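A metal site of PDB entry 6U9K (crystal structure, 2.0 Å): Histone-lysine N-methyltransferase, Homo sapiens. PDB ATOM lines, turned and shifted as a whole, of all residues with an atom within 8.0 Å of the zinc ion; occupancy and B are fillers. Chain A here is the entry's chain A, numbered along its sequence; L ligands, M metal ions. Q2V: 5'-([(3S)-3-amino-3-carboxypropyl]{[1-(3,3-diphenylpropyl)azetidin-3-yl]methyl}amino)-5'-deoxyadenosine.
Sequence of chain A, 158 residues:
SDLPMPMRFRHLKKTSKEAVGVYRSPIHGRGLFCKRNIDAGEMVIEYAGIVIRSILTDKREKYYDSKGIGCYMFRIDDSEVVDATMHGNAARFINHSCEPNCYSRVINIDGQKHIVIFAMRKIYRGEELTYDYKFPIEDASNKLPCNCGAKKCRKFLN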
ATOM      1  N   ILE A  27      12.645   7.510   8.994  1.00  0.00           N
ATOM      2  CA  ILE A  27      13.602   6.815   8.124  1.00  0.00           C
ATOM      3  C   ILE A  27      12.853   5.608   7.513  1.00  0.00           C
ATOM      4  O   ILE A  27      12.700   5.550   6.296  1.00  0.00           O
ATOM      5  CB  ILE A  27      14.906   6.412   8.880  1.00  0.00           C
ATOM      6  CG1 ILE A  27      15.731   7.649   9.289  1.00  0.00           C
ATOM      7  CG2 ILE A  27      15.747   5.469   8.000  1.00  0.00           C
ATOM      8  CD1 ILE A  27      16.821   7.387  10.430  1.00  0.00           C
ATOM      9  N   HIS A  96      19.283   2.007   9.741  1.00  0.00           N
ATOM     10  CA  HIS A  96      20.566   2.396   9.149  1.00  0.00           C
ATOM     11  C   HIS A  96      20.658   3.912   8.951  1.00  0.00           C
ATOM     12  O   HIS A  96      19.651   4.546   8.619  1.00  0.00           O
ATOM     13  CB  HIS A  96      20.753   1.723   7.753  1.00  0.00           C
ATOM     14  CG  HIS A  96      21.881   2.308   6.970  1.00  0.00           C
ATOM     15  ND1 HIS A  96      23.181   1.936   7.200  1.00  0.00           N
ATOM     16  CD2 HIS A  96      21.870   3.315   6.063  1.00  0.00           C
ATOM     17  CE1 HIS A  96      23.922   2.687   6.408  1.00  0.00           C
ATOM     18  NE2 HIS A  96      23.181   3.546   5.718  1.00  0.00           N
ATOM     19  N   SER A  97      21.876   4.470   9.064  1.00  0.00           N
ATOM     20  CA  SER A  97      22.176   5.872   8.724  1.00  0.00           C
ATOM     21  C   SER A  97      23.589   6.007   8.242  1.00  0.00           C
ATOM     22  O   SER A  97      24.471   5.296   8.730  1.00  0.00           O
ATOM     23  CB  SER A  97      21.944   6.818   9.893  1.00  0.00           C
ATOM     24  OG  SER A  97      22.277   8.147   9.522  1.00  0.00           O
ATOM     25  N   CYS A  98      23.820   6.977   7.304  1.00  0.00           N
ATOM     26  CA  CYS A  98      25.129   7.257   6.716  1.00  0.00           C
ATOM     27  C   CYS A  98      25.910   8.233   7.564  1.00  0.00           C
ATOM     28  O   CYS A  98      27.122   8.402   7.372  1.00  0.00           O
ATOM     29  CB  CYS A  98      24.983   7.727   5.274  1.00  0.00           C
ATOM     30  SG  CYS A  98      24.015   6.602   4.243  1.00  0.00           S
ATOM     31  N   GLU A  99      25.226   8.855   8.527  1.00  0.00           N
ATOM     32  CA  GLU A  99      25.816   9.719   9.532  1.00  0.00           C
ATOM     33  C   GLU A  99      25.274   9.083  10.822  1.00  0.00           C
ATOM     34  O   GLU A  99      24.354   9.637  11.425  1.00  0.00           O
ATOM     35  CB  GLU A  99      25.338  11.173   9.349  1.00  0.00           C
ATOM     36  CG  GLU A  99      25.708  12.093  10.511  1.00  0.00           C
ATOM     37  CD  GLU A  99      26.846  13.032  10.202  1.00  0.00           C
ATOM     38  OE1 GLU A  99      27.619  13.361  11.135  1.00  0.00           O
ATOM     39  OE2 GLU A  99      26.953  13.459   9.034  1.00  0.00           O
ATOM     40  N   PRO A 145      17.280   1.771  -1.552  1.00  0.00           N
ATOM     41  CA  PRO A 145      17.556   3.210  -1.361  1.00  0.00           C
ATOM     42  C   PRO A 145      17.573   3.656   0.103  1.00  0.00           C
ATOM     43  O   PRO A 145      16.743   3.187   0.885  1.00  0.00           O
ATOM     44  CB  PRO A 145      16.442   3.904  -2.166  1.00  0.00           C
ATOM     45  CG  PRO A 145      15.371   2.871  -2.326  1.00  0.00           C
ATOM     46  CD  PRO A 145      16.075   1.553  -2.383  1.00  0.00           C
ATOM     47  N   CYS A 146      18.540   4.506   0.493  1.00  0.00           N
ATOM     48  CA  CYS A 146      18.663   4.992   1.863  1.00  0.00           C
ATOM     49  C   CYS A 146      17.825   6.214   2.107  1.00  0.00           C
ATOM     50  O   CYS A 146      17.865   7.169   1.308  1.00  0.00           O
ATOM     51  CB  CYS A 146      20.115   5.235   2.250  1.00  0.00           C
ATOM     52  SG  CYS A 146      20.353   5.572   4.008  1.00  0.00           S
ATOM     53  N   ASN A 147      17.133   6.240   3.255  1.00  0.00           N
ATOM     54  CA  ASN A 147      16.255   7.329   3.669  1.00  0.00           C
ATOM     55  C   ASN A 147      16.739   7.995   4.980  1.00  0.00           C
ATOM     56  O   ASN A 147      15.934   8.588   5.703  1.00  0.00           O
ATOM     57  CB  ASN A 147      14.807   6.819   3.792  1.00  0.00           C
ATOM     58  CG  ASN A 147      13.745   7.903   3.736  1.00  0.00           C
ATOM     59  OD1 ASN A 147      13.801   8.842   2.935  1.00  0.00           O
ATOM     60  ND2 ASN A 147      12.750   7.786   4.589  1.00  0.00           N
ATOM     61  N   CYS A 148      18.053   7.915   5.278  1.00  0.00           N
ATOM     62  CA  CYS A 148      18.597   8.526   6.509  1.00  0.00           C
ATOM     63  C   CYS A 148      18.536  10.060   6.458  1.00  0.00           C
ATOM     64  O   CYS A 148      18.449  10.701   7.514  1.00  0.00           O
ATOM     65  CB  CYS A 148      20.004   8.006   6.809  1.00  0.00           C
ATOM     66  SG  CYS A 148      21.315   8.754   5.801  1.00  0.00           S
ATOM     67  N   GLY A 149      18.583  10.616   5.240  1.00  0.00           N
ATOM     68  CA  GLY A 149      18.499  12.040   4.969  1.00  0.00           C
ATOM     69  C   GLY A 149      19.754  12.836   5.246  1.00  0.00           C
ATOM     70  O   GLY A 149      19.721  14.067   5.152  1.00  0.00           O
ATOM     71  N   ALA A 150      20.879  12.159   5.559  1.00  0.00           N
ATOM     72  CA  ALA A 150      22.154  12.838   5.861  1.00  0.00           C
ATOM     73  C   ALA A 150      22.697  13.610   4.649  1.00  0.00           C
ATOM     74  O   ALA A 150      22.397  13.233   3.509  1.00  0.00           O
ATOM     75  CB  ALA A 150      23.194  11.834   6.338  1.00  0.00           C
ATOM     76  N   LYS A 151      23.477  14.672   4.889  1.00  0.00           N
ATOM     77  CA  LYS A 151      24.082  15.423   3.783  1.00  0.00           C
ATOM     78  C   LYS A 151      25.015  14.472   2.989  1.00  0.00           C
ATOM     79  O   LYS A 151      24.936  14.413   1.765  1.00  0.00           O
ATOM     80  CB  LYS A 151      24.853  16.640   4.308  1.00  0.00           C
ATOM     81  CG  LYS A 151      25.374  17.569   3.204  1.00  0.00           C
ATOM     82  N   LYS A 152      25.851  13.702   3.713  1.00  0.00           N
ATOM     83  CA  LYS A 152      26.835  12.764   3.170  1.00  0.00           C
ATOM     84  C   LYS A 152      26.252  11.359   2.930  1.00  0.00           C
ATOM     85  O   LYS A 152      26.985  10.371   2.995  1.00  0.00           O
ATOM     86  CB  LYS A 152      28.071  12.728   4.103  1.00  0.00           C
ATOM     87  N   CYS A 153      24.936  11.275   2.646  1.00  0.00           N
ATOM     88  CA  CYS A 153      24.229  10.017   2.412  1.00  0.00           C
ATOM     89  C   CYS A 153      24.798   9.261   1.222  1.00  0.00           C
ATOM     90  O   CYS A 153      25.036   9.865   0.189  1.00  0.00           O
ATOM     91  CB  CYS A 153      22.726  10.264   2.258  1.00  0.00           C
ATOM     92  SG  CYS A 153      21.738   8.763   2.001  1.00  0.00           S
ATOM     93  N   ARG A 154      25.036   7.928   1.377  1.00  0.00           N
ATOM     94  CA  ARG A 154      25.548   7.058   0.312  1.00  0.00           C
ATOM     95  C   ARG A 154      24.409   6.640  -0.639  1.00  0.00           C
ATOM     96  O   ARG A 154      24.646   5.962  -1.620  1.00  0.00           O
ATOM     97  CB  ARG A 154      26.293   5.836   0.898  1.00  0.00           C
ATOM     98  N   LYS A 155      23.165   7.053  -0.299  1.00  0.00           N
ATOM     99  CA  LYS A 155      21.914   6.891  -1.054  1.00  0.00           C
ATOM    100  C   LYS A 155      21.408   5.451  -1.213  1.00  0.00           C
ATOM    101  O   LYS A 155      20.290   5.265  -1.709  1.00  0.00           O
ATOM    102  CB  LYS A 155      22.000   7.608  -2.418  1.00  0.00           C
ATOM    103  CG  LYS A 155      22.389   9.107  -2.316  1.00  0.00           C
ATOM    104  CD  LYS A 155      21.343   9.989  -1.622  1.00  0.00           C
ATOM    105  CE  LYS A 155      21.662  11.464  -1.744  1.00  0.00           C
ATOM    106  NZ  LYS A 155      20.514  12.312  -1.322  1.00  0.00           N
ATOM    107  N   PHE A 156      22.207   4.445  -0.778  1.00  0.00           N
ATOM    108  CA  PHE A 156      21.853   3.022  -0.805  1.00  0.00           C
ATOM    109  C   PHE A 156      22.383   2.296   0.426  1.00  0.00           C
ATOM    110  O   PHE A 156      23.439   2.653   0.958  1.00  0.00           O
ATOM    111  CB  PHE A 156      22.351   2.322  -2.094  1.00  0.00           C
ATOM    112  CG  PHE A 156      21.748   2.910  -3.352  1.00  0.00           C
ATOM    113  CD1 PHE A 156      20.466   2.573  -3.753  1.00  0.00           C
ATOM    114  CD2 PHE A 156      22.448   3.879  -4.074  1.00  0.00           C
ATOM    115  CE1 PHE A 156      19.893   3.170  -4.882  1.00  0.00           C
ATOM    116  CE2 PHE A 156      21.869   4.482  -5.198  1.00  0.00           C
ATOM    117  CZ  PHE A 156      20.590   4.128  -5.595  1.00  0.00           C
ATOM    118  N   LEU A 157      21.630   1.274   0.882  1.00  0.00           N
ATOM    119  CA  LEU A 157      21.994   0.434   2.017  1.00  0.00           C
ATOM    120  C   LEU A 157      22.979  -0.631   1.548  1.00  0.00           C
ATOM    121  O   LEU A 157      22.973  -0.984   0.370  1.00  0.00           O
ATOM    122  CB  LEU A 157      20.740  -0.233   2.598  1.00  0.00           C
ATOM    123  CG  LEU A 157      20.197   0.342   3.899  1.00  0.00           C
ATOM    124  CD1 LEU A 157      19.688   1.771   3.707  1.00  0.00           C
ATOM    125  CD2 LEU A 157      19.085  -0.531   4.444  1.00  0.00           C
HETATM  126  N1  Q2V L   1      16.679   3.738   4.587  1.00  0.00           N
HETATM  127  C2  Q2V L   1      15.839   1.471   5.869  1.00  0.00           C
HETATM  128  C3  Q2V L   1      16.863   2.246   6.483  1.00  0.00           C
HETATM  129  O4  Q2V L   1      14.582  -1.504   7.615  1.00  0.00           O
HETATM  130  C6  Q2V L   1      15.397  -1.677   5.345  1.00  0.00           C
HETATM  131  C8  Q2V L   1      15.109  -2.801   7.428  1.00  0.00           C
HETATM  132  C9  Q2V L   1      15.793  -3.218   8.747  1.00  0.00           C
HETATM  133  C10 Q2V L   1      14.490  -4.698  10.327  1.00  0.00           C
HETATM  134  C11 Q2V L   1      13.819  -5.466   9.163  1.00  0.00           C
HETATM  135  C12 Q2V L   1      12.541  -4.812   8.521  1.00  0.00           C
HETATM  136  C13 Q2V L   1      10.440  -6.067   9.175  1.00  0.00           C
HETATM  137  C16 Q2V L   1       7.572  -3.794   7.984  1.00  0.00           C
HETATM  138  C17 Q2V L   1       7.566  -3.724   6.577  1.00  0.00           C
HETATM  139  C18 Q2V L   1       7.093  -2.583   5.930  1.00  0.00           C
HETATM  140  C19 Q2V L   1       6.604  -1.490   6.674  1.00  0.00           C
HETATM  141  C20 Q2V L   1       6.583  -1.561   8.069  1.00  0.00           C
HETATM  142  C21 Q2V L   1       7.059  -2.705   8.724  1.00  0.00           C
HETATM  143  C22 Q2V L   1       7.311  -6.177   8.771  1.00  0.00           C
HETATM  144  C23 Q2V L   1       6.511  -6.379   9.914  1.00  0.00           C
HETATM  145  C24 Q2V L   1       5.681  -7.512  10.022  1.00  0.00           C
HETATM  146  C25 Q2V L   1       5.627  -8.449   8.981  1.00  0.00           C
HETATM  147  C26 Q2V L   1       6.419  -8.267   7.833  1.00  0.00           C
HETATM  148  C27 Q2V L   1       7.246  -7.130   7.716  1.00  0.00           C
HETATM  149  C28 Q2V L   1      12.904  -6.595   9.582  1.00  0.00           C
HETATM  150  C29 Q2V L   1      14.928  -2.257  10.909  1.00  0.00           C
HETATM  151  C30 Q2V L   1      13.574  -2.011  11.673  1.00  0.00           C
HETATM  152  O3  Q2V L   1      10.139  -1.302  11.507  1.00  0.00           O
HETATM  153  C32 Q2V L   1      11.083  -1.998  11.228  1.00  0.00           C
HETATM  154  O2  Q2V L   1      10.921  -3.320  11.384  1.00  0.00           O
HETATM  155  C31 Q2V L   1      12.459  -1.562  10.699  1.00  0.00           C
HETATM  156  N7  Q2V L   1      12.415  -0.098  10.613  1.00  0.00           N
HETATM  157  N5  Q2V L   1      14.743  -3.303   9.853  1.00  0.00           N
HETATM  158  C7  Q2V L   1      16.116  -2.714   6.224  1.00  0.00           C
HETATM  159  O1  Q2V L   1      16.163  -3.910   5.544  1.00  0.00           O
HETATM  160  O   Q2V L   1      14.292  -2.163   4.664  1.00  0.00           O
HETATM  161  C5  Q2V L   1      14.758  -0.740   6.453  1.00  0.00           C
HETATM  162  N4  Q2V L   1      15.632   0.397   6.721  1.00  0.00           N
HETATM  163  N2  Q2V L   1      15.217   1.769   4.673  1.00  0.00           N
HETATM  164  C1  Q2V L   1      15.698   2.904   4.118  1.00  0.00           C
HETATM  165  C4  Q2V L   1      16.523   0.565   7.817  1.00  0.00           C
HETATM  166  N3  Q2V L   1      17.282   1.671   7.692  1.00  0.00           N
HETATM  167  C   Q2V L   1      17.271   3.414   5.774  1.00  0.00           C
HETATM  168  N   Q2V L   1      18.250   4.235   6.274  1.00  0.00           N
HETATM  169  N6  Q2V L   1      11.827  -6.128   8.634  1.00  0.00           N
HETATM  170  C14 Q2V L   1       9.613  -5.228   8.177  1.00  0.00           C
HETATM  171  C15 Q2V L   1       8.214  -4.948   8.742  1.00  0.00           C
HETATM  172 ZN    ZN M   1      21.906   7.408   4.016  1.00  0.00          ZN
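The zinc ion is bound by the side-chain sulfur of Cys 98, the side-chain sulfur of Cys 148, the side-chain sulfur of Cys 146 and the side-chain sulfur of Cys 153.
The side-chain sulfur (SG) of Cys 146 lies close to a nitrogen (N) of the ligand (3.4 Å). The backbone carbonyl oxygen (O) of His 96 lies within hydrogen-bond range of a nitrogen (N) of the ligand (2.7 Å). The backbone NH of His 96 is in hydrogen-bond range of a nitrogen (N3) of the ligand (2.9 Å). The backbone NH (N) of Asn 147 lies within hydrogen-bond range of a nitrogen (N1) of the ligand.
The backbone NH (N) of Arg 154 lies close to the side-chain sulfur (SG) of Cys 98. SG of Cys 153 sits close to N of Lys 155 (3.2 Å). The backbone NH of Cys 146 is in hydrogen-bond range of the backbone carbonyl oxygen of Lys 155, at 2.9 Å. The side-chain sulfur of Cys 148 lies close to the backbone NH of Ala 150, 3.4 Å away. The side-chain sulfur (SG) of Cys 98 lies close to a ring nitrogen (NE2) of His 96, at 3.5 Å.
Of the 18 residues printed, 4 come within 4 Å of the zinc ion. Along chain A the residues within 4 Å of the zinc ion span positions 98 to 153.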
